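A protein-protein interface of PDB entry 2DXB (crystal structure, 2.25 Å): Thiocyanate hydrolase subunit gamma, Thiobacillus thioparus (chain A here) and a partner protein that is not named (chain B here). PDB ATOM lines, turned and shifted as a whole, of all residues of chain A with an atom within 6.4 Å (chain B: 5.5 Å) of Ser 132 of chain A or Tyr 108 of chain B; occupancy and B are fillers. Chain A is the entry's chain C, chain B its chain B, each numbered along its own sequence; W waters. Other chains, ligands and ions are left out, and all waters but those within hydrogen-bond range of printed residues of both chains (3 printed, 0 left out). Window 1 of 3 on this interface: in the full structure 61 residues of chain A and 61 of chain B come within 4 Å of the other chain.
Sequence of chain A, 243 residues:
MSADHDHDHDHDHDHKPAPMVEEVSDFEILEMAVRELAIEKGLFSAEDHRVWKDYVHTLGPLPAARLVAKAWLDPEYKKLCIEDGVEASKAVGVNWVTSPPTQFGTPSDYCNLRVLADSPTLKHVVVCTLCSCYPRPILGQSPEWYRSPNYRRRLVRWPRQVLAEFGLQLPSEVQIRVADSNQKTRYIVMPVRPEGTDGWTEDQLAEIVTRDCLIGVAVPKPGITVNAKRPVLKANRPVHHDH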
ATOM      1  N   CYS A 128       9.266  13.568 -26.889  1.00  0.00           N
ATOM      2  CA  CYS A 128      10.670  13.962 -26.948  1.00  0.00           C
ATOM      3  C   CYS A 128      11.046  14.077 -25.481  1.00  0.00           C
ATOM      4  O   CYS A 128      10.856  15.136 -24.871  1.00  0.00           O
ATOM      5  CB  CYS A 128      10.850  15.317 -27.633  1.00  0.00           C
ATOM      6  SG  CYS A 128      12.584  15.916 -27.615  1.00  0.00           S
ATOM      7  N   THR A 129      11.562  12.994 -24.906  1.00  0.00           N
ATOM      8  CA  THR A 129      11.910  13.012 -23.488  1.00  0.00           C
ATOM      9  C   THR A 129      13.019  14.009 -23.158  1.00  0.00           C
ATOM     10  O   THR A 129      13.092  14.500 -22.032  1.00  0.00           O
ATOM     11  CB  THR A 129      12.343  11.618 -22.973  1.00  0.00           C
ATOM     12  OG1 THR A 129      13.581  11.234 -23.589  1.00  0.00           O
ATOM     13  CG2 THR A 129      11.268  10.575 -23.287  1.00  0.00           C
ATOM     14  N   LEU A 130      13.864  14.322 -24.137  1.00  0.00           N
ATOM     15  CA  LEU A 130      14.962  15.257 -23.912  1.00  0.00           C
ATOM     16  C   LEU A 130      14.526  16.725 -23.911  1.00  0.00           C
ATOM     17  O   LEU A 130      15.220  17.584 -23.318  1.00  0.00           O
ATOM     18  CB  LEU A 130      16.060  15.053 -24.954  1.00  0.00           C
ATOM     19  CG  LEU A 130      16.736  13.679 -24.892  1.00  0.00           C
ATOM     20  CD1 LEU A 130      17.847  13.592 -25.930  1.00  0.00           C
ATOM     21  CD2 LEU A 130      17.290  13.442 -23.490  1.00  0.00           C
ATOM     22  N   CSD A 131      13.390  17.008 -24.554  1.00  0.00           N
ATOM     23  CA  CSD A 131      12.861  18.362 -24.629  1.00  0.00           C
ATOM     24  CB  CSD A 131      13.814  19.358 -25.286  1.00  0.00           C
ATOM     25  SG  CSD A 131      14.391  18.845 -26.946  1.00  0.00           S
ATOM     26  C   CSD A 131      11.440  18.529 -25.155  1.00  0.00           C
ATOM     27  O   CSD A 131      10.471  18.328 -24.415  1.00  0.00           O
ATOM     28  OD1 CSD A 131      15.128  19.930 -27.497  1.00  0.00           O
ATOM     29  OD2 CSD A 131      15.294  17.654 -26.832  1.00  0.00           O
ATOM     30  N   SER A 132      11.314  18.918 -26.424  1.00  0.00           N
ATOM     31  CA  SER A 132       9.995  19.123 -27.014  1.00  0.00           C
ATOM     32  C   SER A 132       9.972  18.947 -28.518  1.00  0.00           C
ATOM     33  O   SER A 132       9.044  19.379 -29.191  1.00  0.00           O
ATOM     34  CB  SER A 132       9.478  20.515 -26.632  1.00  0.00           C
ATOM     35  OG  SER A 132      10.425  21.530 -26.946  1.00  0.00           O
ATOM     36  N   CSO A 133      11.002  18.305 -29.048  1.00  0.00           N
ATOM     37  CA  CSO A 133      11.076  18.058 -30.481  1.00  0.00           C
ATOM     38  CB  CSO A 133      12.229  17.134 -30.863  1.00  0.00           C
ATOM     39  SG  CSO A 133      13.787  17.668 -30.072  1.00  0.00           S
ATOM     40  C   CSO A 133       9.731  17.665 -31.087  1.00  0.00           C
ATOM     41  O   CSO A 133       9.111  16.681 -30.681  1.00  0.00           O
ATOM     42  OD  CSO A 133      14.040  18.945 -30.818  1.00  0.00           O
ATOM     43  N   TYR A 134       9.267  18.459 -32.042  1.00  0.00           N
ATOM     44  CA  TYR A 134       7.952  18.301 -32.657  1.00  0.00           C
ATOM     45  C   TYR A 134       8.068  18.629 -34.155  1.00  0.00           C
ATOM     46  O   TYR A 134       8.865  19.486 -34.537  1.00  0.00           O
ATOM     47  CB  TYR A 134       7.036  19.301 -31.943  1.00  0.00           C
ATOM     48  CG  TYR A 134       5.548  19.157 -32.104  1.00  0.00           C
ATOM     49  CD1 TYR A 134       4.841  18.180 -31.402  1.00  0.00           C
ATOM     50  CD2 TYR A 134       4.826  20.079 -32.868  1.00  0.00           C
ATOM     51  CE1 TYR A 134       3.452  18.140 -31.448  1.00  0.00           C
ATOM     52  CE2 TYR A 134       3.446  20.043 -32.917  1.00  0.00           C
ATOM     53  CZ  TYR A 134       2.765  19.078 -32.204  1.00  0.00           C
ATOM     54  OH  TYR A 134       1.389  19.088 -32.228  1.00  0.00           O
ATOM     55  N   PRO A 135       7.277  17.960 -35.017  1.00  0.00           N
ATOM     56  CA  PRO A 135       7.323  18.209 -36.467  1.00  0.00           C
ATOM     57  C   PRO A 135       6.602  19.512 -36.844  1.00  0.00           C
ATOM     58  O   PRO A 135       5.623  19.503 -37.602  1.00  0.00           O
ATOM     59  CB  PRO A 135       6.627  16.980 -37.041  1.00  0.00           C
ATOM     60  CG  PRO A 135       5.560  16.717 -36.017  1.00  0.00           C
ATOM     61  CD  PRO A 135       6.316  16.886 -34.700  1.00  0.00           C
ATOM     62  N   ARG A 136       7.099  20.630 -36.323  1.00  0.00           N
ATOM     63  CA  ARG A 136       6.497  21.939 -36.555  1.00  0.00           C
ATOM     64  C   ARG A 136       6.112  22.280 -38.006  1.00  0.00           C
ATOM     65  O   ARG A 136       4.978  22.675 -38.275  1.00  0.00           O
ATOM     66  CB  ARG A 136       7.412  23.047 -36.014  1.00  0.00           C
ATOM     67  CG  ARG A 136       7.681  23.028 -34.502  1.00  0.00           C
ATOM     68  CD  ARG A 136       8.268  24.383 -34.080  1.00  0.00           C
ATOM     69  NE  ARG A 136       8.593  24.473 -32.658  1.00  0.00           N
ATOM     70  CZ  ARG A 136       9.718  24.015 -32.111  1.00  0.00           C
ATOM     71  NH1 ARG A 136      10.640  23.423 -32.865  1.00  0.00           N
ATOM     72  NH2 ARG A 136       9.934  24.174 -30.810  1.00  0.00           N
ATOM     73  N   GLN A 141       2.847  24.359 -33.813  1.00  0.00           N
ATOM     74  CA  GLN A 141       3.506  24.470 -32.518  1.00  0.00           C
ATOM     75  C   GLN A 141       3.092  23.329 -31.578  1.00  0.00           C
ATOM     76  O   GLN A 141       1.968  22.831 -31.638  1.00  0.00           O
ATOM     77  CB  GLN A 141       3.171  25.836 -31.907  1.00  0.00           C
ATOM     78  CG  GLN A 141       4.123  26.321 -30.826  1.00  0.00           C
ATOM     79  CD  GLN A 141       5.571  26.390 -31.290  1.00  0.00           C
ATOM     80  OE1 GLN A 141       6.293  25.382 -31.284  1.00  0.00           O
ATOM     81  NE2 GLN A 141       6.004  27.580 -31.697  1.00  0.00           N
ATOM     82  N   SER A 142       4.015  22.914 -30.716  1.00  0.00           N
ATOM     83  CA  SER A 142       3.758  21.826 -29.781  1.00  0.00           C
ATOM     84  C   SER A 142       2.827  22.223 -28.635  1.00  0.00           C
ATOM     85  O   SER A 142       2.813  23.374 -28.200  1.00  0.00           O
ATOM     86  CB  SER A 142       5.082  21.310 -29.204  1.00  0.00           C
ATOM     87  OG  SER A 142       5.764  22.328 -28.480  1.00  0.00           O
ATOM     88  N   GLU A 144       1.338  22.605 -24.872  1.00  0.00           N
ATOM     89  CA  GLU A 144       2.025  22.915 -23.622  1.00  0.00           C
ATOM     90  C   GLU A 144       2.341  21.632 -22.846  1.00  0.00           C
ATOM     91  O   GLU A 144       3.437  21.481 -22.315  1.00  0.00           O
ATOM     92  CB  GLU A 144       1.160  23.845 -22.758  1.00  0.00           C
ATOM     93  CG  GLU A 144       1.750  24.170 -21.388  1.00  0.00           C
ATOM     94  CD  GLU A 144       2.930  25.137 -21.445  1.00  0.00           C
ATOM     95  OE1 GLU A 144       3.362  25.515 -22.560  1.00  0.00           O
ATOM     96  OE2 GLU A 144       3.425  25.525 -20.362  1.00  0.00           O
ATOM     97  N   TYR A 146       2.843  18.679 -23.998  1.00  0.00           N
ATOM     98  CA  TYR A 146       3.838  17.886 -24.713  1.00  0.00           C
ATOM     99  C   TYR A 146       5.245  18.255 -24.223  1.00  0.00           C
ATOM    100  O   TYR A 146       6.162  17.426 -24.245  1.00  0.00           O
ATOM    101  CB  TYR A 146       3.736  18.163 -26.216  1.00  0.00           C
ATOM    102  CG  TYR A 146       4.643  17.307 -27.078  1.00  0.00           C
ATOM    103  CD1 TYR A 146       4.275  16.014 -27.446  1.00  0.00           C
ATOM    104  CD2 TYR A 146       5.867  17.796 -27.530  1.00  0.00           C
ATOM    105  CE1 TYR A 146       5.105  15.227 -28.250  1.00  0.00           C
ATOM    106  CE2 TYR A 146       6.704  17.016 -28.333  1.00  0.00           C
ATOM    107  CZ  TYR A 146       6.314  15.734 -28.689  1.00  0.00           C
ATOM    108  OH  TYR A 146       7.131  14.969 -29.487  1.00  0.00           O
ATOM    109  N   ARG A 147       5.400  19.502 -23.776  1.00  0.00           N
ATOM    110  CA  ARG A 147       6.685  20.012 -23.293  1.00  0.00           C
ATOM    111  C   ARG A 147       6.931  19.780 -21.798  1.00  0.00           C
ATOM    112  O   ARG A 147       8.030  20.025 -21.304  1.00  0.00           O
ATOM    113  CB  ARG A 147       6.776  21.524 -23.542  1.00  0.00           C
ATOM    114  CG  ARG A 147       6.320  21.996 -24.915  1.00  0.00           C
ATOM    115  CD  ARG A 147       6.141  23.510 -24.935  1.00  0.00           C
ATOM    116  NE  ARG A 147       5.623  23.978 -26.220  1.00  0.00           N
ATOM    117  CZ  ARG A 147       5.228  25.224 -26.463  1.00  0.00           C
ATOM    118  NH1 ARG A 147       5.290  26.142 -25.506  1.00  0.00           N
ATOM    119  NH2 ARG A 147       4.752  25.550 -27.661  1.00  0.00           N
ATOM    120  N   ARG A 152       7.089  13.912 -20.532  1.00  0.00           N
ATOM    121  CA  ARG A 152       8.406  13.447 -20.947  1.00  0.00           C
ATOM    122  C   ARG A 152       8.965  12.357 -20.038  1.00  0.00           C
ATOM    123  O   ARG A 152       9.758  11.523 -20.472  1.00  0.00           O
ATOM    124  CB  ARG A 152       9.364  14.637 -21.010  1.00  0.00           C
ATOM    125  CG  ARG A 152       8.973  15.665 -22.067  1.00  0.00           C
ATOM    126  CD  ARG A 152       9.767  16.951 -21.888  1.00  0.00           C
ATOM    127  NE  ARG A 152      11.180  16.658 -21.717  1.00  0.00           N
ATOM    128  CZ  ARG A 152      12.009  17.396 -20.989  1.00  0.00           C
ATOM    129  NH1 ARG A 152      11.564  18.484 -20.373  1.00  0.00           N
ATOM    130  NH2 ARG A 152      13.267  17.013 -20.838  1.00  0.00           N
ATOM    131  N   ARG A 186      11.720  13.678 -36.885  1.00  0.00           N
ATOM    132  CA  ARG A 186      10.476  14.147 -36.289  1.00  0.00           C
ATOM    133  C   ARG A 186       9.389  13.210 -36.814  1.00  0.00           C
ATOM    134  O   ARG A 186       9.469  12.733 -37.947  1.00  0.00           O
ATOM    135  CB  ARG A 186      10.198  15.594 -36.702  1.00  0.00           C
ATOM    136  CG  ARG A 186      11.261  16.589 -36.218  1.00  0.00           C
ATOM    137  CD  ARG A 186      11.281  16.739 -34.699  1.00  0.00           C
ATOM    138  NE  ARG A 186      12.312  17.683 -34.259  1.00  0.00           N
ATOM    139  CZ  ARG A 186      13.572  17.354 -33.980  1.00  0.00           C
ATOM    140  NH1 ARG A 186      13.977  16.091 -34.085  1.00  0.00           N
ATOM    141  NH2 ARG A 186      14.435  18.292 -33.603  1.00  0.00           N
ATOM    142  N   GLN B  94      20.778  25.439 -23.393  1.00  0.00           N
ATOM    143  CA  GLN B  94      19.444  25.689 -22.871  1.00  0.00           C
ATOM    144  C   GLN B  94      18.832  24.620 -21.968  1.00  0.00           C
ATOM    145  O   GLN B  94      18.220  24.936 -20.945  1.00  0.00           O
ATOM    146  CB  GLN B  94      18.512  25.936 -24.059  1.00  0.00           C
ATOM    147  CG  GLN B  94      17.055  26.126 -23.720  1.00  0.00           C
ATOM    148  CD  GLN B  94      16.183  26.095 -24.965  1.00  0.00           C
ATOM    149  OE1 GLN B  94      16.308  26.948 -25.847  1.00  0.00           O
ATOM    150  NE2 GLN B  94      15.300  25.099 -25.046  1.00  0.00           N
ATOM    151  N   MET B 106      12.510  27.256 -13.448  1.00  0.00           N
ATOM    152  CA  MET B 106      12.111  28.322 -14.362  1.00  0.00           C
ATOM    153  C   MET B 106      11.193  27.804 -15.472  1.00  0.00           C
ATOM    154  O   MET B 106      11.075  26.594 -15.679  1.00  0.00           O
ATOM    155  CB  MET B 106      13.358  28.982 -14.960  1.00  0.00           C
ATOM    156  CG  MET B 106      14.080  29.923 -13.994  1.00  0.00           C
ATOM    157  SD  MET B 106      13.095  31.406 -13.601  1.00  0.00           S
ATOM    158  CE  MET B 106      13.600  32.473 -14.957  1.00  0.00           C
ATOM    159  N   PRO B 107      10.510  28.719 -16.184  1.00  0.00           N
ATOM    160  CA  PRO B 107       9.606  28.323 -17.269  1.00  0.00           C
ATOM    161  C   PRO B 107      10.348  27.899 -18.537  1.00  0.00           C
ATOM    162  O   PRO B 107      11.448  28.368 -18.813  1.00  0.00           O
ATOM    163  CB  PRO B 107       8.768  29.584 -17.516  1.00  0.00           C
ATOM    164  CG  PRO B 107       8.912  30.380 -16.251  1.00  0.00           C
ATOM    165  CD  PRO B 107      10.353  30.152 -15.884  1.00  0.00           C
ATOM    166  N   TYR B 108       9.716  27.009 -19.293  1.00  0.00           N
ATOM    167  CA  TYR B 108      10.222  26.495 -20.561  1.00  0.00           C
ATOM    168  C   TYR B 108      10.857  27.614 -21.405  1.00  0.00           C
ATOM    169  O   TYR B 108      12.068  27.611 -21.639  1.00  0.00           O
ATOM    170  CB  TYR B 108       9.044  25.856 -21.301  1.00  0.00           C
ATOM    171  CG  TYR B 108       9.289  25.401 -22.722  1.00  0.00           C
ATOM    172  CD1 TYR B 108       9.857  24.154 -22.995  1.00  0.00           C
ATOM    173  CD2 TYR B 108       8.858  26.180 -23.797  1.00  0.00           C
ATOM    174  CE1 TYR B 108       9.975  23.694 -24.311  1.00  0.00           C
ATOM    175  CE2 TYR B 108       8.974  25.731 -25.107  1.00  0.00           C
ATOM    176  CZ  TYR B 108       9.528  24.488 -25.356  1.00  0.00           C
ATOM    177  OH  TYR B 108       9.601  24.041 -26.655  1.00  0.00           O
ATOM    178  N   TYR B 109      10.045  28.572 -21.854  1.00  0.00           N
ATOM    179  CA  TYR B 109      10.564  29.674 -22.664  1.00  0.00           C
ATOM    180  C   TYR B 109      11.491  30.617 -21.903  1.00  0.00           C
ATOM    181  O   TYR B 109      12.270  31.354 -22.509  1.00  0.00           O
ATOM    182  CB  TYR B 109       9.414  30.461 -23.304  1.00  0.00           C
ATOM    183  CG  TYR B 109       9.027  29.913 -24.664  1.00  0.00           C
ATOM    184  CD1 TYR B 109       7.726  29.487 -24.931  1.00  0.00           C
ATOM    185  CD2 TYR B 109       9.986  29.783 -25.673  1.00  0.00           C
ATOM    186  CE1 TYR B 109       7.390  28.940 -26.179  1.00  0.00           C
ATOM    187  CE2 TYR B 109       9.665  29.239 -26.913  1.00  0.00           C
ATOM    188  CZ  TYR B 109       8.369  28.819 -27.156  1.00  0.00           C
ATOM    189  OH  TYR B 109       8.076  28.275 -28.378  1.00  0.00           O
ATOM    190  N   GLY B 110      11.410  30.596 -20.576  1.00  0.00           N
ATOM    191  CA  GLY B 110      12.297  31.435 -19.794  1.00  0.00           C
ATOM    192  C   GLY B 110      13.722  30.955 -20.030  1.00  0.00           C
ATOM    193  O   GLY B 110      14.655  31.748 -20.092  1.00  0.00           O
ATOM    194  N   ARG B 111      13.887  29.643 -20.177  1.00  0.00           N
ATOM    195  CA  ARG B 111      15.209  29.071 -20.420  1.00  0.00           C
ATOM    196  C   ARG B 111      15.668  29.380 -21.846  1.00  0.00           C
ATOM    197  O   ARG B 111      16.855  29.628 -22.082  1.00  0.00           O
ATOM    198  CB  ARG B 111      15.185  27.560 -20.165  1.00  0.00           C
ATOM    199  CG  ARG B 111      14.929  27.224 -18.703  1.00  0.00           C
ATOM    200  CD  ARG B 111      15.034  25.737 -18.404  1.00  0.00           C
ATOM    201  NE  ARG B 111      13.999  24.950 -19.067  1.00  0.00           N
ATOM    202  CZ  ARG B 111      14.163  24.295 -20.212  1.00  0.00           C
ATOM    203  NH1 ARG B 111      15.333  24.324 -20.842  1.00  0.00           N
ATOM    204  NH2 ARG B 111      13.157  23.598 -20.722  1.00  0.00           N
ATOM    205  N   TRP B 112      14.725  29.371 -22.788  1.00  0.00           N
ATOM    206  CA  TRP B 112      15.034  29.690 -24.178  1.00  0.00           C
ATOM    207  C   TRP B 112      15.607  31.102 -24.226  1.00  0.00           C
ATOM    208  O   TRP B 112      16.644  31.346 -24.843  1.00  0.00           O
ATOM    209  CB  TRP B 112      13.769  29.662 -25.042  1.00  0.00           C
ATOM    210  CG  TRP B 112      13.301  28.301 -25.487  1.00  0.00           C
ATOM    211  CD1 TRP B 112      12.783  27.307 -24.707  1.00  0.00           C
ATOM    212  CD2 TRP B 112      13.281  27.809 -26.834  1.00  0.00           C
ATOM    213  NE1 TRP B 112      12.435  26.224 -25.486  1.00  0.00           N
ATOM    214  CE2 TRP B 112      12.733  26.504 -26.794  1.00  0.00           C
ATOM    215  CE3 TRP B 112      13.674  28.343 -28.071  1.00  0.00           C
ATOM    216  CZ2 TRP B 112      12.567  25.723 -27.950  1.00  0.00           C
ATOM    217  CZ3 TRP B 112      13.512  27.567 -29.220  1.00  0.00           C
ATOM    218  CH2 TRP B 112      12.962  26.269 -29.150  1.00  0.00           C
HETATM  219  O   HOH W   1       8.218  25.582 -28.893  1.00  0.00           O
HETATM  220  O   HOH W   2      12.600  22.718 -25.679  1.00  0.00           O
HETATM  221  O   HOH W   3      14.691  22.583 -26.958  1.00  0.00           O
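The side-chain hydroxyl (OH) of Tyr 108 of chain B is in hydrogen-bond range of the side-chain hydroxyl (OG) of Ser 132 of chain A (2.7 Å).
The guanidinium group (NE) of Arg 136 of chain A sits at hydrogen-bond distance from the side-chain amide oxygen (OE1) of Gln 141 of chain A.
The side-chain hydroxyl (OG) of Ser 142 of chain A is in hydrogen-bond range of the guanidinium group (NE) of Arg 147 of chain A (2.8 Å).
NH1 of Arg 147 of chain A lies within salt-bridge range of OE1 of Glu 144 of chain A (3.6 Å).
Among the printed residues, merely in contact across the chains: Arg 147 of chain A with Tyr 108 of chain B (3.6 Å), Arg 147 of chain A with Tyr 109 of chain B (3.6 Å) and Gln 141 of chain A with Tyr 109 of chain B (3.97 Å).
Of chain B, only Tyr 108 (2.7 Å) comes within 4 Å of Ser 132 of chain A.
Pro 135 of chain A touches none of the printed residues of chain B.
Arg 136 of chain A touches none of the printed residues of chain B.
Printed residues of chain B within 4 Å of Gln 141 of chain A: Tyr 109 (3.97 Å).
Printed residues of chain B within 4 Å of Arg 147 of chain A: Tyr 108 (3.6 Å) and Tyr 109 (3.6 Å).
Tyr 108 of chain B touches just these residues of chain A: Ser 132 and Arg 147.
Printed residues of chain A within 4 Å of Tyr 109 of chain B: Gln 141 (3.97 Å) and Arg 147 (3.6 Å).
The nearest residue of chain A that does not touch Tyr 108 of chain B is Arg 136 of chain A (4.2 Å).
Hydrophobic or aromatic side chains of chain B that line the printed part of chain A: Tyr 108 and Tyr 109.
Along chain B the printed residues that touch a printed residue of chain A span positions 108 to 109.
Of the 16 printed residues of chain A, 3 touch a printed residue of chain B.
Among the printed residues, no Asp or Glu carboxylate lies within 4 Å of a Lys or Arg side-chain nitrogen of the other chain.
Water W3 bridges OD1 of CSD 131 of chain A and NE2 of Gln 94 of chain B.
Water W1 lies within hydrogen-bond range of OH of Tyr 109 of chain B (2.7 Å), NH2 of Arg 136 of chain A (2.9 Å), OH of Tyr 108 of chain B (3.0 Å) and OE1 of Gln 141 of chain A (3.1 Å).
Water W2 lies within hydrogen-bond range of OG of Ser 132 of chain A (2.8 Å) and OH of Tyr 108 of chain B (3.4 Å).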
